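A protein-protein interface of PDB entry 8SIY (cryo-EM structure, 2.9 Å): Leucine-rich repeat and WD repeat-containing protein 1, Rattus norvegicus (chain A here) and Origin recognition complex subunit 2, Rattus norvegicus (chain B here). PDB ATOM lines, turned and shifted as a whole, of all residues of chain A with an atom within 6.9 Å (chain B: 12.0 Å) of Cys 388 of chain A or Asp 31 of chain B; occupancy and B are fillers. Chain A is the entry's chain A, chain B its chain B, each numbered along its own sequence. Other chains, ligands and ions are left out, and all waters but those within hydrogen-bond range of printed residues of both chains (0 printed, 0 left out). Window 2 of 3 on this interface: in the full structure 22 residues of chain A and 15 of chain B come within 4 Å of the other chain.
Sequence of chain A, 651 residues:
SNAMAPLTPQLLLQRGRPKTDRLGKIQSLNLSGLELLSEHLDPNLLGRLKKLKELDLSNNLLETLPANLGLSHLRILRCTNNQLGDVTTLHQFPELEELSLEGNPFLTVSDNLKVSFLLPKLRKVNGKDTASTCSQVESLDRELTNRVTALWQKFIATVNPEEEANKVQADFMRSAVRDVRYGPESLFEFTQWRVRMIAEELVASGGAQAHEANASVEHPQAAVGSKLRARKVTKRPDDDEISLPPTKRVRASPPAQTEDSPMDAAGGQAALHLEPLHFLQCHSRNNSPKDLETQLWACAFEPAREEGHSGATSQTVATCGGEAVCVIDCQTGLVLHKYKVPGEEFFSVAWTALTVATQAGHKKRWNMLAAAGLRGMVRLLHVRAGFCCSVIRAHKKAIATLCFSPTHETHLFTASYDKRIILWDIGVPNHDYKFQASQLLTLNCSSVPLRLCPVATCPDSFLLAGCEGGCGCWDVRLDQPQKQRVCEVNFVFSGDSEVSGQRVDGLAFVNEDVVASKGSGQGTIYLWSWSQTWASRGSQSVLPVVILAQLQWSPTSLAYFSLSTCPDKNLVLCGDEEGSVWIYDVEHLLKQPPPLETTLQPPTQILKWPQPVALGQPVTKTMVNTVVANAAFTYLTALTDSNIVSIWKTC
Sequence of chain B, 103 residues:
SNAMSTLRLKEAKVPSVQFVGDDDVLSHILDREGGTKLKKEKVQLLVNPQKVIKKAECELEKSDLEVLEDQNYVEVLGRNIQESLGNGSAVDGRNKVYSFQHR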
ATOM      1  N   TYR A 339     -32.384 -19.284 -15.858  1.00  0.00           N
ATOM      2  CA  TYR A 339     -32.192 -18.053 -16.604  1.00  0.00           C
ATOM      3  C   TYR A 339     -33.383 -17.901 -17.536  1.00  0.00           C
ATOM      4  O   TYR A 339     -33.700 -18.832 -18.281  1.00  0.00           O
ATOM      5  CB  TYR A 339     -30.891 -18.099 -17.409  1.00  0.00           C
ATOM      6  CG  TYR A 339     -30.629 -16.870 -18.234  1.00  0.00           C
ATOM      7  CD1 TYR A 339     -30.579 -15.618 -17.654  1.00  0.00           C
ATOM      8  CD2 TYR A 339     -30.403 -16.970 -19.595  1.00  0.00           C
ATOM      9  CE1 TYR A 339     -30.325 -14.494 -18.405  1.00  0.00           C
ATOM     10  CE2 TYR A 339     -30.148 -15.854 -20.358  1.00  0.00           C
ATOM     11  CZ  TYR A 339     -30.110 -14.617 -19.759  1.00  0.00           C
ATOM     12  OH  TYR A 339     -29.856 -13.500 -20.518  1.00  0.00           O
ATOM     13  N   LYS A 340     -34.031 -16.738 -17.496  1.00  0.00           N
ATOM     14  CA  LYS A 340     -35.211 -16.445 -18.296  1.00  0.00           C
ATOM     15  C   LYS A 340     -34.954 -15.246 -19.203  1.00  0.00           C
ATOM     16  O   LYS A 340     -34.427 -14.241 -18.733  1.00  0.00           O
ATOM     17  CB  LYS A 340     -36.371 -16.172 -17.337  1.00  0.00           C
ATOM     18  CG  LYS A 340     -36.514 -17.235 -16.245  1.00  0.00           C
ATOM     19  CD  LYS A 340     -37.907 -17.286 -15.684  1.00  0.00           C
ATOM     20  CE  LYS A 340     -38.829 -17.925 -16.663  1.00  0.00           C
ATOM     21  NZ  LYS A 340     -40.143 -18.097 -16.039  1.00  0.00           N
ATOM     22  N   VAL A 341     -35.286 -15.375 -20.494  1.00  0.00           N
ATOM     23  CA  VAL A 341     -35.257 -14.259 -21.439  1.00  0.00           C
ATOM     24  C   VAL A 341     -36.608 -14.185 -22.131  1.00  0.00           C
ATOM     25  O   VAL A 341     -37.106 -15.187 -22.651  1.00  0.00           O
ATOM     26  CB  VAL A 341     -34.116 -14.419 -22.468  1.00  0.00           C
ATOM     27  CG1 VAL A 341     -32.811 -14.685 -21.748  1.00  0.00           C
ATOM     28  CG2 VAL A 341     -34.389 -15.549 -23.451  1.00  0.00           C
ATOM     29  N   PRO A 342     -37.298 -13.010 -22.108  1.00  0.00           N
ATOM     30  CA  PRO A 342     -38.678 -12.925 -22.613  1.00  0.00           C
ATOM     31  C   PRO A 342     -38.826 -13.342 -24.058  1.00  0.00           C
ATOM     32  O   PRO A 342     -38.127 -12.852 -24.942  1.00  0.00           O
ATOM     33  CB  PRO A 342     -39.018 -11.434 -22.456  1.00  0.00           C
ATOM     34  CG  PRO A 342     -37.675 -10.730 -22.048  1.00  0.00           C
ATOM     35  CD  PRO A 342     -37.004 -11.809 -21.296  1.00  0.00           C
ATOM     36  N   MET A 368     -18.311 -23.039 -18.837  1.00  0.00           N
ATOM     37  CA  MET A 368     -19.333 -22.140 -19.350  1.00  0.00           C
ATOM     38  C   MET A 368     -20.451 -22.927 -20.016  1.00  0.00           C
ATOM     39  O   MET A 368     -20.241 -24.020 -20.550  1.00  0.00           O
ATOM     40  CB  MET A 368     -18.731 -21.148 -20.345  1.00  0.00           C
ATOM     41  CG  MET A 368     -17.962 -20.011 -19.694  1.00  0.00           C
ATOM     42  SD  MET A 368     -19.038 -18.836 -18.847  1.00  0.00           S
ATOM     43  CE  MET A 368     -19.115 -17.495 -20.037  1.00  0.00           C
ATOM     44  N   VAL A 378     -26.750 -16.151 -29.321  1.00  0.00           N
ATOM     45  CA  VAL A 378     -26.032 -17.135 -28.521  1.00  0.00           C
ATOM     46  C   VAL A 378     -25.669 -16.491 -27.194  1.00  0.00           C
ATOM     47  O   VAL A 378     -24.907 -15.518 -27.156  1.00  0.00           O
ATOM     48  CB  VAL A 378     -24.776 -17.637 -29.249  1.00  0.00           C
ATOM     49  CG1 VAL A 378     -24.062 -18.686 -28.412  1.00  0.00           C
ATOM     50  CG2 VAL A 378     -25.136 -18.187 -30.621  1.00  0.00           C
ATOM     51  N   ARG A 379     -26.209 -17.028 -26.108  1.00  0.00           N
ATOM     52  CA  ARG A 379     -25.965 -16.512 -24.769  1.00  0.00           C
ATOM     53  C   ARG A 379     -25.079 -17.492 -24.019  1.00  0.00           C
ATOM     54  O   ARG A 379     -25.463 -18.646 -23.806  1.00  0.00           O
ATOM     55  CB  ARG A 379     -27.275 -16.291 -24.020  1.00  0.00           C
ATOM     56  CG  ARG A 379     -28.229 -15.349 -24.715  1.00  0.00           C
ATOM     57  CD  ARG A 379     -29.368 -14.953 -23.805  1.00  0.00           C
ATOM     58  NE  ARG A 379     -30.415 -14.251 -24.534  1.00  0.00           N
ATOM     59  CZ  ARG A 379     -31.350 -14.850 -25.257  1.00  0.00           C
ATOM     60  NH1 ARG A 379     -31.418 -16.168 -25.345  1.00  0.00           N
ATOM     61  NH2 ARG A 379     -32.237 -14.108 -25.914  1.00  0.00           N
ATOM     62  N   LEU A 380     -23.903 -17.030 -23.619  1.00  0.00           N
ATOM     63  CA  LEU A 380     -22.970 -17.824 -22.837  1.00  0.00           C
ATOM     64  C   LEU A 380     -23.122 -17.434 -21.374  1.00  0.00           C
ATOM     65  O   LEU A 380     -22.882 -16.278 -21.008  1.00  0.00           O
ATOM     66  CB  LEU A 380     -21.537 -17.604 -23.312  1.00  0.00           C
ATOM     67  CG  LEU A 380     -20.951 -18.687 -24.216  1.00  0.00           C
ATOM     68  CD1 LEU A 380     -21.739 -18.808 -25.505  1.00  0.00           C
ATOM     69  CD2 LEU A 380     -19.490 -18.386 -24.505  1.00  0.00           C
ATOM     70  N   LEU A 381     -23.521 -18.393 -20.549  1.00  0.00           N
ATOM     71  CA  LEU A 381     -23.835 -18.154 -19.147  1.00  0.00           C
ATOM     72  C   LEU A 381     -22.774 -18.802 -18.274  1.00  0.00           C
ATOM     73  O   LEU A 381     -22.460 -19.985 -18.447  1.00  0.00           O
ATOM     74  CB  LEU A 381     -25.213 -18.720 -18.801  1.00  0.00           C
ATOM     75  CG  LEU A 381     -26.314 -18.488 -19.840  1.00  0.00           C
ATOM     76  CD1 LEU A 381     -27.588 -19.212 -19.432  1.00  0.00           C
ATOM     77  CD2 LEU A 381     -26.577 -17.005 -20.032  1.00  0.00           C
ATOM     78  N   HIS A 382     -22.223 -18.031 -17.339  1.00  0.00           N
ATOM     79  CA  HIS A 382     -21.324 -18.574 -16.322  1.00  0.00           C
ATOM     80  C   HIS A 382     -22.206 -19.057 -15.177  1.00  0.00           C
ATOM     81  O   HIS A 382     -22.514 -18.318 -14.241  1.00  0.00           O
ATOM     82  CB  HIS A 382     -20.309 -17.530 -15.876  1.00  0.00           C
ATOM     83  CG  HIS A 382     -19.233 -18.073 -14.987  1.00  0.00           C
ATOM     84  ND1 HIS A 382     -19.288 -19.335 -14.434  1.00  0.00           N
ATOM     85  CD2 HIS A 382     -18.069 -17.528 -14.561  1.00  0.00           C
ATOM     86  CE1 HIS A 382     -18.207 -19.541 -13.703  1.00  0.00           C
ATOM     87  NE2 HIS A 382     -17.450 -18.460 -13.763  1.00  0.00           N
ATOM     88  N   GLY A 386     -23.220 -17.375 -11.659  1.00  0.00           N
ATOM     89  CA  GLY A 386     -24.589 -16.932 -11.500  1.00  0.00           C
ATOM     90  C   GLY A 386     -25.025 -15.752 -12.344  1.00  0.00           C
ATOM     91  O   GLY A 386     -25.934 -15.021 -11.936  1.00  0.00           O
ATOM     92  N   PHE A 387     -24.419 -15.537 -13.511  1.00  0.00           N
ATOM     93  CA  PHE A 387     -24.858 -14.445 -14.371  1.00  0.00           C
ATOM     94  C   PHE A 387     -24.451 -14.723 -15.810  1.00  0.00           C
ATOM     95  O   PHE A 387     -23.558 -15.530 -16.083  1.00  0.00           O
ATOM     96  CB  PHE A 387     -24.292 -13.098 -13.908  1.00  0.00           C
ATOM     97  CG  PHE A 387     -22.790 -13.057 -13.834  1.00  0.00           C
ATOM     98  CD1 PHE A 387     -22.030 -12.835 -14.969  1.00  0.00           C
ATOM     99  CD2 PHE A 387     -22.142 -13.220 -12.622  1.00  0.00           C
ATOM    100  CE1 PHE A 387     -20.653 -12.790 -14.899  1.00  0.00           C
ATOM    101  CE2 PHE A 387     -20.765 -13.175 -12.547  1.00  0.00           C
ATOM    102  CZ  PHE A 387     -20.021 -12.960 -13.687  1.00  0.00           C
ATOM    103  N   CYS A 388     -25.128 -14.033 -16.727  1.00  0.00           N
ATOM    104  CA  CYS A 388     -24.835 -14.128 -18.152  1.00  0.00           C
ATOM    105  C   CYS A 388     -23.684 -13.192 -18.498  1.00  0.00           C
ATOM    106  O   CYS A 388     -23.759 -11.985 -18.245  1.00  0.00           O
ATOM    107  CB  CYS A 388     -26.075 -13.777 -18.972  1.00  0.00           C
ATOM    108  SG  CYS A 388     -25.804 -13.761 -20.758  1.00  0.00           S
ATOM    109  N   CYS A 389     -22.623 -13.746 -19.086  1.00  0.00           N
ATOM    110  CA  CYS A 389     -21.429 -12.956 -19.366  1.00  0.00           C
ATOM    111  C   CYS A 389     -21.597 -12.109 -20.620  1.00  0.00           C
ATOM    112  O   CYS A 389     -21.414 -10.888 -20.581  1.00  0.00           O
ATOM    113  CB  CYS A 389     -20.217 -13.877 -19.502  1.00  0.00           C
ATOM    114  SG  CYS A 389     -19.671 -14.606 -17.943  1.00  0.00           S
ATOM    115  N   SER A 390     -21.940 -12.737 -21.743  1.00  0.00           N
ATOM    116  CA  SER A 390     -22.023 -12.030 -23.012  1.00  0.00           C
ATOM    117  C   SER A 390     -23.105 -12.663 -23.872  1.00  0.00           C
ATOM    118  O   SER A 390     -23.611 -13.747 -23.574  1.00  0.00           O
ATOM    119  CB  SER A 390     -20.681 -12.044 -23.755  1.00  0.00           C
ATOM    120  OG  SER A 390     -19.704 -11.289 -23.060  1.00  0.00           O
ATOM    121  N   VAL A 391     -23.466 -11.953 -24.937  1.00  0.00           N
ATOM    122  CA  VAL A 391     -24.457 -12.407 -25.902  1.00  0.00           C
ATOM    123  C   VAL A 391     -23.915 -12.150 -27.300  1.00  0.00           C
ATOM    124  O   VAL A 391     -23.374 -11.072 -27.571  1.00  0.00           O
ATOM    125  CB  VAL A 391     -25.809 -11.698 -25.709  1.00  0.00           C
ATOM    126  CG1 VAL A 391     -26.813 -12.177 -26.745  1.00  0.00           C
ATOM    127  CG2 VAL A 391     -26.328 -11.937 -24.303  1.00  0.00           C
ATOM    128  N   TYR A 433     -15.289 -10.232 -17.638  1.00  0.00           N
ATOM    129  CA  TYR A 433     -16.284 -11.200 -18.103  1.00  0.00           C
ATOM    130  C   TYR A 433     -16.899 -10.800 -19.444  1.00  0.00           C
ATOM    131  O   TYR A 433     -18.089 -11.023 -19.678  1.00  0.00           O
ATOM    132  CB  TYR A 433     -17.392 -11.392 -17.062  1.00  0.00           C
ATOM    133  CG  TYR A 433     -16.930 -11.976 -15.744  1.00  0.00           C
ATOM    134  CD1 TYR A 433     -16.311 -11.184 -14.786  1.00  0.00           C
ATOM    135  CD2 TYR A 433     -17.129 -13.319 -15.450  1.00  0.00           C
ATOM    136  CE1 TYR A 433     -15.894 -11.713 -13.580  1.00  0.00           C
ATOM    137  CE2 TYR A 433     -16.719 -13.856 -14.244  1.00  0.00           C
ATOM    138  CZ  TYR A 433     -16.099 -13.050 -13.314  1.00  0.00           C
ATOM    139  OH  TYR A 433     -15.686 -13.581 -12.113  1.00  0.00           O
ATOM    140  N   SER B  27     -30.882 -20.603  -7.059  1.00  0.00           N
ATOM    141  CA  SER B  27     -30.257 -19.364  -7.496  1.00  0.00           C
ATOM    142  C   SER B  27     -30.800 -18.985  -8.865  1.00  0.00           C
ATOM    143  O   SER B  27     -31.060 -19.856  -9.698  1.00  0.00           O
ATOM    144  CB  SER B  27     -28.731 -19.497  -7.564  1.00  0.00           C
ATOM    145  OG  SER B  27     -28.133 -18.271  -7.942  1.00  0.00           O
ATOM    146  N   HIS B  28     -30.960 -17.687  -9.093  1.00  0.00           N
ATOM    147  CA  HIS B  28     -31.345 -17.160 -10.393  1.00  0.00           C
ATOM    148  C   HIS B  28     -30.116 -16.610 -11.106  1.00  0.00           C
ATOM    149  O   HIS B  28     -29.297 -15.915 -10.499  1.00  0.00           O
ATOM    150  CB  HIS B  28     -32.390 -16.048 -10.257  1.00  0.00           C
ATOM    151  CG  HIS B  28     -33.713 -16.504  -9.721  1.00  0.00           C
ATOM    152  ND1 HIS B  28     -34.796 -16.761 -10.535  1.00  0.00           N
ATOM    153  CD2 HIS B  28     -34.137 -16.717  -8.453  1.00  0.00           C
ATOM    154  CE1 HIS B  28     -35.827 -17.123  -9.792  1.00  0.00           C
ATOM    155  NE2 HIS B  28     -35.454 -17.106  -8.525  1.00  0.00           N
ATOM    156  N   ILE B  29     -29.988 -16.931 -12.386  1.00  0.00           N
ATOM    157  CA  ILE B  29     -28.985 -16.302 -13.236  1.00  0.00           C
ATOM    158  C   ILE B  29     -29.484 -14.920 -13.636  1.00  0.00           C
ATOM    159  O   ILE B  29     -30.652 -14.752 -14.007  1.00  0.00           O
ATOM    160  CB  ILE B  29     -28.712 -17.167 -14.479  1.00  0.00           C
ATOM    161  CG1 ILE B  29     -28.328 -18.594 -14.076  1.00  0.00           C
ATOM    162  CG2 ILE B  29     -27.635 -16.534 -15.352  1.00  0.00           C
ATOM    163  CD1 ILE B  29     -27.107 -18.684 -13.189  1.00  0.00           C
ATOM    164  N   LEU B  30     -28.605 -13.923 -13.564  1.00  0.00           N
ATOM    165  CA  LEU B  30     -28.964 -12.551 -13.889  1.00  0.00           C
ATOM    166  C   LEU B  30     -28.158 -12.066 -15.086  1.00  0.00           C
ATOM    167  O   LEU B  30     -27.125 -12.638 -15.443  1.00  0.00           O
ATOM    168  CB  LEU B  30     -28.731 -11.615 -12.698  1.00  0.00           C
ATOM    169  CG  LEU B  30     -29.455 -11.953 -11.393  1.00  0.00           C
ATOM    170  CD1 LEU B  30     -30.884 -12.407 -11.660  1.00  0.00           C
ATOM    171  CD2 LEU B  30     -28.686 -12.995 -10.590  1.00  0.00           C
ATOM    172  N   ASP B  31     -28.646 -10.997 -15.706  1.00  0.00           N
ATOM    173  CA  ASP B  31     -27.989 -10.430 -16.874  1.00  0.00           C
ATOM    174  C   ASP B  31     -26.757  -9.634 -16.468  1.00  0.00           C
ATOM    175  O   ASP B  31     -25.639  -9.964 -16.862  1.00  0.00           O
ATOM    176  CB  ASP B  31     -28.958  -9.538 -17.656  1.00  0.00           C
ATOM    177  CG  ASP B  31     -30.148 -10.307 -18.198  1.00  0.00           C
ATOM    178  OD1 ASP B  31     -29.981 -11.495 -18.545  1.00  0.00           O
ATOM    179  OD2 ASP B  31     -31.249  -9.724 -18.277  1.00  0.00           O
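The side-chain hydroxyl (OH) of Tyr 339 of chain A is in hydrogen-bond range of the side-chain carboxylate (OD1) of Asp 31 of chain B, 2.8 Å away. The backbone carbonyl oxygen (O) of Gly 386 of chain A lies within hydrogen-bond range of the backbone NH (N) of Leu 30 of chain B. N of Cys 388 of chain A sits at hydrogen-bond distance from O of Leu 30 of chain B (2.8 Å). O of Cys 388 of chain A sits close to O of Asp 31 of chain B.
Hydrophobic or aromatic side chains of chain A that line the printed part of chain B: Tyr 339 and Phe 387. Of the 5 printed residues of chain B, 4 touch a printed residue of chain A. Hydrophobic or aromatic side chains of chain B within 4 Å of the printed part of chain A: Ile 29 and Leu 30. Among the printed residues, 10 pairs touch across the chains. Among the printed residues, no Asp or Glu carboxylate lies within 4 Å of a Lys or Arg side-chain nitrogen of the other chain.
Among the printed residues, merely in contact across the chains: Phe 387 of chain A with Leu 30 of chain B (3.1 Å), Gly 386 of chain A with Ile 29 of chain B (3.5 Å), Phe 387 of chain A with Ile 29 of chain B (3.6 Å), Tyr 339 of chain A with Ile 29 of chain B (3.7 Å), Gly 386 of chain A with His 28 of chain B (3.8 Å) and Cys 388 of chain A with Ile 29 of chain B (3.8 Å).
Of chain A, only Tyr 339 and Cys 388 come within 4 Å of Asp 31 of chain B. No residue of chain B comes within 4 Å of Leu 381 of chain A. Phe 387 of chain A touches just these residues of chain B: Ile 29 (3.6 Å) and Leu 30 (3.1 Å). Cys 389 of chain A touches none of the printed residues of chain B. No residue of chain B comes within 4 Å of Ser 390 of chain A. Of the printed residues of chain A, Ile 29 of chain B touches Tyr 339 (3.7 Å), Gly 386 (3.5 Å), Phe 387 (3.6 Å) and Cys 388 (3.8 Å). Printed residues of chain B within 4 Å of Tyr 339 of chain A: Ile 29 (3.7 Å) and Asp 31 (2.8 Å). Printed residues of chain A within 4 Å of Leu 30 of chain B: Gly 386 (3.3 Å), Phe 387 (3.1 Å) and Cys 388 (2.8 Å). Printed residues of chain A within 4 Å of His 28 of chain B: Gly 386 (3.8 Å). The nearest residue of chain A that does not touch Asp 31 of chain B is Phe 387 of chain A (4.5 Å).
N of His 382 of chain A sits at hydrogen-bond distance from O of Phe 387 of chain A. The side-chain sulfur (SG) of Cys 388 of chain A sits at hydrogen-bond distance from the backbone carbonyl oxygen (O) of Ser 390 of chain A, 3.6 Å away.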
